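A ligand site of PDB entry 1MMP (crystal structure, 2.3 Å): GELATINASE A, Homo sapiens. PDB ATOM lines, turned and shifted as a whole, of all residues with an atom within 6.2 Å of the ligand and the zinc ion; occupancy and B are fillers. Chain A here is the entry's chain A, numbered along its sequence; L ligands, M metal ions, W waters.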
ATOM      1  N   ASP A  76      12.022   0.488  19.836  1.00  0.00           N
ATOM      2  CA  ASP A  76      11.418  -0.609  20.584  1.00  0.00           C
ATOM      3  C   ASP A  76      12.299  -1.300  21.629  1.00  0.00           C
ATOM      4  O   ASP A  76      12.072  -2.478  21.929  1.00  0.00           O
ATOM      5  CB  ASP A  76      10.949  -1.614  19.496  1.00  0.00           C
ATOM      6  CG  ASP A  76      12.154  -2.021  18.621  1.00  0.00           C
ATOM      7  OD1 ASP A  76      13.309  -1.649  18.866  1.00  0.00           O
ATOM      8  OD2 ASP A  76      11.977  -2.717  17.626  1.00  0.00           O
ATOM      9  N   GLY A  79      17.439  -4.916  20.731  1.00  0.00           N
ATOM     10  CA  GLY A  79      17.121  -5.837  19.642  1.00  0.00           C
ATOM     11  C   GLY A  79      16.039  -5.331  18.717  1.00  0.00           C
ATOM     12  O   GLY A  79      15.657  -4.151  18.764  1.00  0.00           O
ATOM     13  N   ASN A  80      15.579  -6.202  17.813  1.00  0.00           N
ATOM     14  CA  ASN A  80      14.550  -5.899  16.812  1.00  0.00           C
ATOM     15  C   ASN A  80      15.030  -4.765  15.942  1.00  0.00           C
ATOM     16  O   ASN A  80      16.105  -4.938  15.372  1.00  0.00           O
ATOM     17  CB  ASN A  80      13.264  -5.601  17.565  1.00  0.00           C
ATOM     18  CG  ASN A  80      12.622  -6.903  17.910  1.00  0.00           C
ATOM     19  OD1 ASN A  80      11.416  -6.974  18.082  1.00  0.00           O
ATOM     20  ND2 ASN A  80      13.305  -8.036  18.079  1.00  0.00           N
ATOM     21  N   THR A  81      14.341  -3.652  15.723  1.00  0.00           N
ATOM     22  CA  THR A  81      14.820  -2.546  14.896  1.00  0.00           C
ATOM     23  C   THR A  81      16.001  -1.928  15.610  1.00  0.00           C
ATOM     24  O   THR A  81      15.912  -1.576  16.785  1.00  0.00           O
ATOM     25  CB  THR A  81      13.680  -1.537  14.731  1.00  0.00           C
ATOM     26  OG1 THR A  81      12.640  -2.220  14.041  1.00  0.00           O
ATOM     27  CG2 THR A  81      14.100  -0.285  13.951  1.00  0.00           C
ATOM     28  N   LEU A  82      17.143  -1.872  14.946  1.00  0.00           N
ATOM     29  CA  LEU A  82      18.392  -1.307  15.475  1.00  0.00           C
ATOM     30  C   LEU A  82      18.515   0.221  15.275  1.00  0.00           C
ATOM     31  O   LEU A  82      19.096   0.948  16.093  1.00  0.00           O
ATOM     32  CB  LEU A  82      19.505  -2.093  14.763  1.00  0.00           C
ATOM     33  CG  LEU A  82      20.175  -3.308  15.425  1.00  0.00           C
ATOM     34  CD1 LEU A  82      19.265  -4.064  16.391  1.00  0.00           C
ATOM     35  CD2 LEU A  82      20.714  -4.137  14.261  1.00  0.00           C
ATOM     36  N   ALA A  83      17.968   0.706  14.158  1.00  0.00           N
ATOM     37  CA  ALA A  83      18.050   2.127  13.772  1.00  0.00           C
ATOM     38  C   ALA A  83      17.136   2.364  12.594  1.00  0.00           C
ATOM     39  O   ALA A  83      16.476   1.405  12.141  1.00  0.00           O
ATOM     40  CB  ALA A  83      19.488   2.414  13.336  1.00  0.00           C
ATOM     41  N   HIS A  84      16.990   3.599  12.128  1.00  0.00           N
ATOM     42  CA  HIS A  84      16.200   3.855  10.925  1.00  0.00           C
ATOM     43  C   HIS A  84      16.662   5.193  10.360  1.00  0.00           C
ATOM     44  O   HIS A  84      17.154   6.059  11.089  1.00  0.00           O
ATOM     45  CB  HIS A  84      14.646   3.876  11.153  1.00  0.00           C
ATOM     46  CG  HIS A  84      14.061   4.753  12.287  1.00  0.00           C
ATOM     47  ND1 HIS A  84      13.181   4.324  13.201  1.00  0.00           N
ATOM     48  CD2 HIS A  84      14.335   6.072  12.544  1.00  0.00           C
ATOM     49  CE1 HIS A  84      12.922   5.314  13.995  1.00  0.00           C
ATOM     50  NE2 HIS A  84      13.608   6.349  13.608  1.00  0.00           N
ATOM     51  N   ALA A  85      16.463   5.404   9.054  1.00  0.00           N
ATOM     52  CA  ALA A  85      16.894   6.642   8.364  1.00  0.00           C
ATOM     53  C   ALA A  85      15.870   6.959   7.278  1.00  0.00           C
ATOM     54  O   ALA A  85      15.064   6.093   6.897  1.00  0.00           O
ATOM     55  CB  ALA A  85      18.278   6.474   7.718  1.00  0.00           C
ATOM     56  N   ILE A 112      26.435  -4.245  18.993  1.00  0.00           N
ATOM     57  CA  ILE A 112      26.103  -3.983  17.589  1.00  0.00           C
ATOM     58  C   ILE A 112      27.159  -3.004  17.099  1.00  0.00           C
ATOM     59  O   ILE A 112      27.419  -1.956  17.684  1.00  0.00           O
ATOM     60  CB  ILE A 112      24.658  -3.383  17.481  1.00  0.00           C
ATOM     61  CG1 ILE A 112      23.620  -4.257  18.235  1.00  0.00           C
ATOM     62  CG2 ILE A 112      24.316  -3.248  15.966  1.00  0.00           C
ATOM     63  CD1 ILE A 112      23.367  -5.659  17.672  1.00  0.00           C
ATOM     64  N   TYR A 116      29.174  -0.572  10.920  1.00  0.00           N
ATOM     65  CA  TYR A 116      28.330  -1.338   9.998  1.00  0.00           C
ATOM     66  C   TYR A 116      26.929  -0.701   9.972  1.00  0.00           C
ATOM     67  O   TYR A 116      26.397  -0.385   8.883  1.00  0.00           O
ATOM     68  CB  TYR A 116      28.266  -2.836  10.463  1.00  0.00           C
ATOM     69  CG  TYR A 116      27.519  -3.604   9.441  1.00  0.00           C
ATOM     70  CD1 TYR A 116      26.117  -3.633   9.471  1.00  0.00           C
ATOM     71  CD2 TYR A 116      28.200  -4.187   8.351  1.00  0.00           C
ATOM     72  CE1 TYR A 116      25.388  -4.217   8.433  1.00  0.00           C
ATOM     73  CE2 TYR A 116      27.478  -4.778   7.311  1.00  0.00           C
ATOM     74  CZ  TYR A 116      26.074  -4.785   7.362  1.00  0.00           C
ATOM     75  OH  TYR A 116      25.364  -5.397   6.339  1.00  0.00           O
ATOM     76  N   ALA A 117      26.320  -0.498  11.159  1.00  0.00           N
ATOM     77  CA  ALA A 117      24.961   0.098  11.224  1.00  0.00           C
ATOM     78  C   ALA A 117      24.900   1.465  10.557  1.00  0.00           C
ATOM     79  O   ALA A 117      24.020   1.751   9.743  1.00  0.00           O
ATOM     80  CB  ALA A 117      24.497   0.256  12.683  1.00  0.00           C
ATOM     81  N   ALA A 118      25.869   2.338  10.840  1.00  0.00           N
ATOM     82  CA  ALA A 118      25.896   3.672  10.243  1.00  0.00           C
ATOM     83  C   ALA A 118      26.066   3.573   8.741  1.00  0.00           C
ATOM     84  O   ALA A 118      25.446   4.365   8.038  1.00  0.00           O
ATOM     85  CB  ALA A 118      27.062   4.531  10.782  1.00  0.00           C
ATOM     86  N   HIS A 120      24.961   1.351   6.698  1.00  0.00           N
ATOM     87  CA  HIS A 120      23.624   0.959   6.224  1.00  0.00           C
ATOM     88  C   HIS A 120      22.648   2.157   6.303  1.00  0.00           C
ATOM     89  O   HIS A 120      21.951   2.473   5.333  1.00  0.00           O
ATOM     90  CB  HIS A 120      23.105  -0.220   7.105  1.00  0.00           C
ATOM     91  CG  HIS A 120      21.771  -0.753   6.568  1.00  0.00           C
ATOM     92  ND1 HIS A 120      21.609  -1.853   5.852  1.00  0.00           N
ATOM     93  CD2 HIS A 120      20.514  -0.196   6.782  1.00  0.00           C
ATOM     94  CE1 HIS A 120      20.313  -1.989   5.614  1.00  0.00           C
ATOM     95  NE2 HIS A 120      19.678  -0.999   6.170  1.00  0.00           N
ATOM     96  N   GLU A 121      22.542   2.792   7.460  1.00  0.00           N
ATOM     97  CA  GLU A 121      21.622   3.914   7.597  1.00  0.00           C
ATOM     98  C   GLU A 121      21.978   5.087   6.710  1.00  0.00           C
ATOM     99  O   GLU A 121      21.111   5.712   6.097  1.00  0.00           O
ATOM    100  CB  GLU A 121      21.562   4.358   9.075  1.00  0.00           C
ATOM    101  CG  GLU A 121      20.925   3.330  10.029  1.00  0.00           C
ATOM    102  CD  GLU A 121      19.656   2.615   9.538  1.00  0.00           C
ATOM    103  OE1 GLU A 121      18.720   3.182   8.935  1.00  0.00           O
ATOM    104  OE2 GLU A 121      19.577   1.415   9.786  1.00  0.00           O
ATOM    105  N   HIS A 124      20.718   4.662   3.286  1.00  0.00           N
ATOM    106  CA  HIS A 124      19.326   5.123   3.185  1.00  0.00           C
ATOM    107  C   HIS A 124      19.327   6.652   3.050  1.00  0.00           C
ATOM    108  O   HIS A 124      18.641   7.187   2.179  1.00  0.00           O
ATOM    109  CB  HIS A 124      18.505   4.730   4.446  1.00  0.00           C
ATOM    110  CG  HIS A 124      18.063   3.283   4.382  1.00  0.00           C
ATOM    111  ND1 HIS A 124      17.556   2.672   3.324  1.00  0.00           N
ATOM    112  CD2 HIS A 124      18.073   2.386   5.434  1.00  0.00           C
ATOM    113  CE1 HIS A 124      17.254   1.441   3.687  1.00  0.00           C
ATOM    114  NE2 HIS A 124      17.561   1.285   4.941  1.00  0.00           N
ATOM    115  N   HIS A 130      16.574  -1.294   0.043  1.00  0.00           N
ATOM    116  CA  HIS A 130      17.144  -2.582   0.442  1.00  0.00           C
ATOM    117  C   HIS A 130      17.543  -3.459  -0.703  1.00  0.00           C
ATOM    118  O   HIS A 130      16.956  -3.435  -1.795  1.00  0.00           O
ATOM    119  CB  HIS A 130      16.165  -3.369   1.313  1.00  0.00           C
ATOM    120  CG  HIS A 130      16.150  -2.753   2.716  1.00  0.00           C
ATOM    121  ND1 HIS A 130      15.112  -2.750   3.547  1.00  0.00           N
ATOM    122  CD2 HIS A 130      17.238  -2.203   3.373  1.00  0.00           C
ATOM    123  CE1 HIS A 130      15.518  -2.236   4.676  1.00  0.00           C
ATOM    124  NE2 HIS A 130      16.793  -1.915   4.555  1.00  0.00           N
ATOM    125  N   VAL A 137      25.651  -4.586   2.037  1.00  0.00           N
ATOM    126  CA  VAL A 137      25.484  -3.821   3.283  1.00  0.00           C
ATOM    127  C   VAL A 137      24.019  -3.406   3.338  1.00  0.00           C
ATOM    128  O   VAL A 137      23.409  -3.394   4.413  1.00  0.00           O
ATOM    129  CB  VAL A 137      26.395  -2.559   3.289  1.00  0.00           C
ATOM    130  CG1 VAL A 137      26.145  -1.755   4.559  1.00  0.00           C
ATOM    131  CG2 VAL A 137      27.869  -2.967   3.294  1.00  0.00           C
ATOM    132  N   MET A 138      23.408  -3.079   2.178  1.00  0.00           N
ATOM    133  CA  MET A 138      21.985  -2.670   2.200  1.00  0.00           C
ATOM    134  C   MET A 138      21.004  -3.814   2.410  1.00  0.00           C
ATOM    135  O   MET A 138      19.780  -3.637   2.264  1.00  0.00           O
ATOM    136  CB  MET A 138      21.632  -1.906   0.923  1.00  0.00           C
ATOM    137  CG  MET A 138      22.341  -0.533   0.881  1.00  0.00           C
ATOM    138  SD  MET A 138      22.301   0.449   2.403  1.00  0.00           S
ATOM    139  CE  MET A 138      20.520   0.581   2.652  1.00  0.00           C
ATOM    140  N   TYR A 139      21.486  -5.014   2.740  1.00  0.00           N
ATOM    141  CA  TYR A 139      20.533  -6.115   3.005  1.00  0.00           C
ATOM    142  C   TYR A 139      19.742  -5.700   4.283  1.00  0.00           C
ATOM    143  O   TYR A 139      20.282  -4.982   5.134  1.00  0.00           O
ATOM    144  CB  TYR A 139      21.313  -7.443   3.231  1.00  0.00           C
ATOM    145  CG  TYR A 139      20.374  -8.585   3.170  1.00  0.00           C
ATOM    146  CD1 TYR A 139      19.802  -8.949   1.941  1.00  0.00           C
ATOM    147  CD2 TYR A 139      20.078  -9.303   4.338  1.00  0.00           C
ATOM    148  CE1 TYR A 139      18.921 -10.025   1.863  1.00  0.00           C
ATOM    149  CE2 TYR A 139      19.193 -10.386   4.271  1.00  0.00           C
ATOM    150  CZ  TYR A 139      18.617 -10.736   3.033  1.00  0.00           C
ATOM    151  OH  TYR A 139      17.701 -11.778   2.964  1.00  0.00           O
ATOM    152  N   PRO A 140      18.463  -6.064   4.436  1.00  0.00           N
ATOM    153  CA  PRO A 140      17.663  -5.621   5.582  1.00  0.00           C
ATOM    154  C   PRO A 140      18.050  -6.072   6.972  1.00  0.00           C
ATOM    155  O   PRO A 140      17.724  -5.361   7.931  1.00  0.00           O
ATOM    156  CB  PRO A 140      16.218  -6.011   5.221  1.00  0.00           C
ATOM    157  CG  PRO A 140      16.414  -7.109   4.208  1.00  0.00           C
ATOM    158  CD  PRO A 140      17.557  -6.577   3.385  1.00  0.00           C
ATOM    159  N   THR A 141      18.648  -7.230   7.176  1.00  0.00           N
ATOM    160  CA  THR A 141      19.034  -7.709   8.504  1.00  0.00           C
ATOM    161  C   THR A 141      20.521  -7.579   8.740  1.00  0.00           C
ATOM    162  O   THR A 141      21.347  -7.555   7.813  1.00  0.00           O
ATOM    163  CB  THR A 141      18.592  -9.171   8.596  1.00  0.00           C
ATOM    164  OG1 THR A 141      19.186  -9.850   7.468  1.00  0.00           O
ATOM    165  CG2 THR A 141      17.057  -9.333   8.550  1.00  0.00           C
ATOM    166  N   TYR A 142      20.875  -7.514  10.012  1.00  0.00           N
ATOM    167  CA  TYR A 142      22.245  -7.404  10.509  1.00  0.00           C
ATOM    168  C   TYR A 142      22.867  -8.781  10.739  1.00  0.00           C
ATOM    169  O   TYR A 142      22.171  -9.703  11.158  1.00  0.00           O
ATOM    170  CB  TYR A 142      22.189  -6.656  11.860  1.00  0.00           C
ATOM    171  CG  TYR A 142      23.467  -6.437  12.518  1.00  0.00           C
ATOM    172  CD1 TYR A 142      24.254  -5.342  12.134  1.00  0.00           C
ATOM    173  CD2 TYR A 142      23.878  -7.303  13.540  1.00  0.00           C
ATOM    174  CE1 TYR A 142      25.464  -5.105  12.790  1.00  0.00           C
ATOM    175  CE2 TYR A 142      25.084  -7.059  14.208  1.00  0.00           C
ATOM    176  CZ  TYR A 142      25.872  -5.963  13.824  1.00  0.00           C
ATOM    177  OH  TYR A 142      27.081  -5.733  14.449  1.00  0.00           O
ATOM    178  N   GLY A 143      24.162  -8.891  10.543  1.00  0.00           N
ATOM    179  CA  GLY A 143      24.943 -10.127  10.810  1.00  0.00           C
ATOM    180  C   GLY A 143      25.069 -11.235   9.785  1.00  0.00           C
ATOM    181  O   GLY A 143      25.409 -12.348  10.175  1.00  0.00           O
HETATM  182  C1  LIG L   1      17.077  -0.699   8.705  1.00  0.00           C
HETATM  183  O1  LIG L   1      17.522   0.531   8.458  1.00  0.00           O
HETATM  184  O2  LIG L   1      16.772  -1.293   7.662  1.00  0.00           O
HETATM  185  C2  LIG L   1      17.058  -1.293  10.095  1.00  0.00           C
HETATM  186  C3  LIG L   1      18.071  -2.427  10.130  1.00  0.00           C
HETATM  187  C4  LIG L   1      17.634  -3.363  11.235  1.00  0.00           C
HETATM  188  O3  LIG L   1      17.591  -2.974  12.398  1.00  0.00           O
HETATM  189  N1  LIG L   1      17.249  -4.594  10.884  1.00  0.00           N
HETATM  190  C5  LIG L   1      16.770  -5.573  11.835  1.00  0.00           C
HETATM  191  C6  LIG L   1      17.878  -6.395  12.413  1.00  0.00           C
HETATM  192  O4  LIG L   1      18.712  -6.881  11.642  1.00  0.00           O
HETATM  193  N2  LIG L   1      17.863  -6.592  13.717  1.00  0.00           N
HETATM  194  C7  LIG L   1      18.841  -7.412  14.434  1.00  0.00           C
HETATM  195  C8  LIG L   1      18.198  -7.813  15.801  1.00  0.00           C
HETATM  196  C9  LIG L   1      16.863  -8.624  15.714  1.00  0.00           C
HETATM  197  C10 LIG L   1      16.965 -10.032  15.134  1.00  0.00           C
HETATM  198  C11 LIG L   1      15.581 -10.746  15.049  1.00  0.00           C
HETATM  199  C12 LIG L   1      14.886 -10.796  13.665  1.00  0.00           C
HETATM  200  N3  LIG L   1      14.710  -9.442  13.135  1.00  0.00           N
HETATM  201  C13 LIG L   1      19.505  -1.910  10.369  1.00  0.00           C
HETATM  202  C14 LIG L   1      20.615  -2.976  10.418  1.00  0.00           C
HETATM  203  C15 LIG L   1      20.768  -3.714   9.071  1.00  0.00           C
HETATM  204  C16 LIG L   1      21.880  -2.255  10.868  1.00  0.00           C
HETATM  205  C17 LIG L   1      15.741  -6.475  11.122  1.00  0.00           C
HETATM  206  C18 LIG L   1      15.135  -7.474  12.036  1.00  0.00           C
HETATM  207  C19 LIG L   1      15.521  -8.804  12.217  1.00  0.00           C
HETATM  208  C20 LIG L   1      14.034  -7.296  12.905  1.00  0.00           C
HETATM  209  C21 LIG L   1      13.800  -8.540  13.561  1.00  0.00           C
HETATM  210  C22 LIG L   1      13.209  -6.184  13.170  1.00  0.00           C
HETATM  211  C23 LIG L   1      12.761  -8.664  14.476  1.00  0.00           C
HETATM  212  C24 LIG L   1      12.175  -6.330  14.074  1.00  0.00           C
HETATM  213  C25 LIG L   1      11.961  -7.566  14.724  1.00  0.00           C
HETATM  214 ZN    ZN M   1      17.593  -0.594   6.004  1.00  0.00          ZN
HETATM  215  O   HOH W   1      14.489   0.527  10.118  1.00  0.00           O
HETATM  216  O   HOH W   2      15.788   2.494   7.892  1.00  0.00           O
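The side-chain carboxylate of Glu 121 sits close to an oxygen (O1) of the ligand, 2.6 Å away. N of Leu 82 lies within hydrogen-bond range of O3 of the ligand (2.8 Å). The backbone carbonyl oxygen (O) of Asn 80 is in hydrogen-bond range of a nitrogen (N2) of the ligand, 2.9 Å away. N1 of the ligand is in hydrogen-bond range of O of Pro 140, 3.1 Å away. N of Tyr 142 sits at hydrogen-bond distance from O4 of the ligand (2.8 Å).
O of Val 137 is in hydrogen-bond range of ND1 of His 120. OE1 of Glu 121 is in hydrogen-bond range of N of Ala 85 (3.2 Å). The backbone carbonyl oxygen of Tyr 139 sits close to a ring nitrogen (ND1) of His 120 (3.5 Å).
Residues that only touch the ligand: Thr 81 (3.7 Å), Ala 83 (3.4 Å), Ala 117 (3.9 Å) and Thr 141 (3.3 Å). Hydrophobic or aromatic side chains within 4 Å of the ligand: Leu 82, His 120, His 124, His 130 and Tyr 142. The nearest printed residue that does not touch the ligand is Tyr 139 (4.2 Å).
Of the 23 residues printed, 3 come within 4 Å of the zinc ion. The nearest printed residue that does not touch the zinc ion is Met 138 (4.6 Å).
The zinc ion is bound by O2 of the ligand, NE2 of His 130, NE2 of His 120 and NE2 of His 124. Slightly farther from the zinc ion lies O1 of the ligand (2.7 Å).
Water W2 lies within hydrogen-bond range of an oxygen (O1) of the ligand (2.7 Å), the side-chain carboxylate of Glu 121 (3.2 Å) and the backbone NH of Ala 85 (3.2 Å). Water W1 bridges the backbone carbonyl oxygen of Ala 83 and an oxygen (O1) of the ligand.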
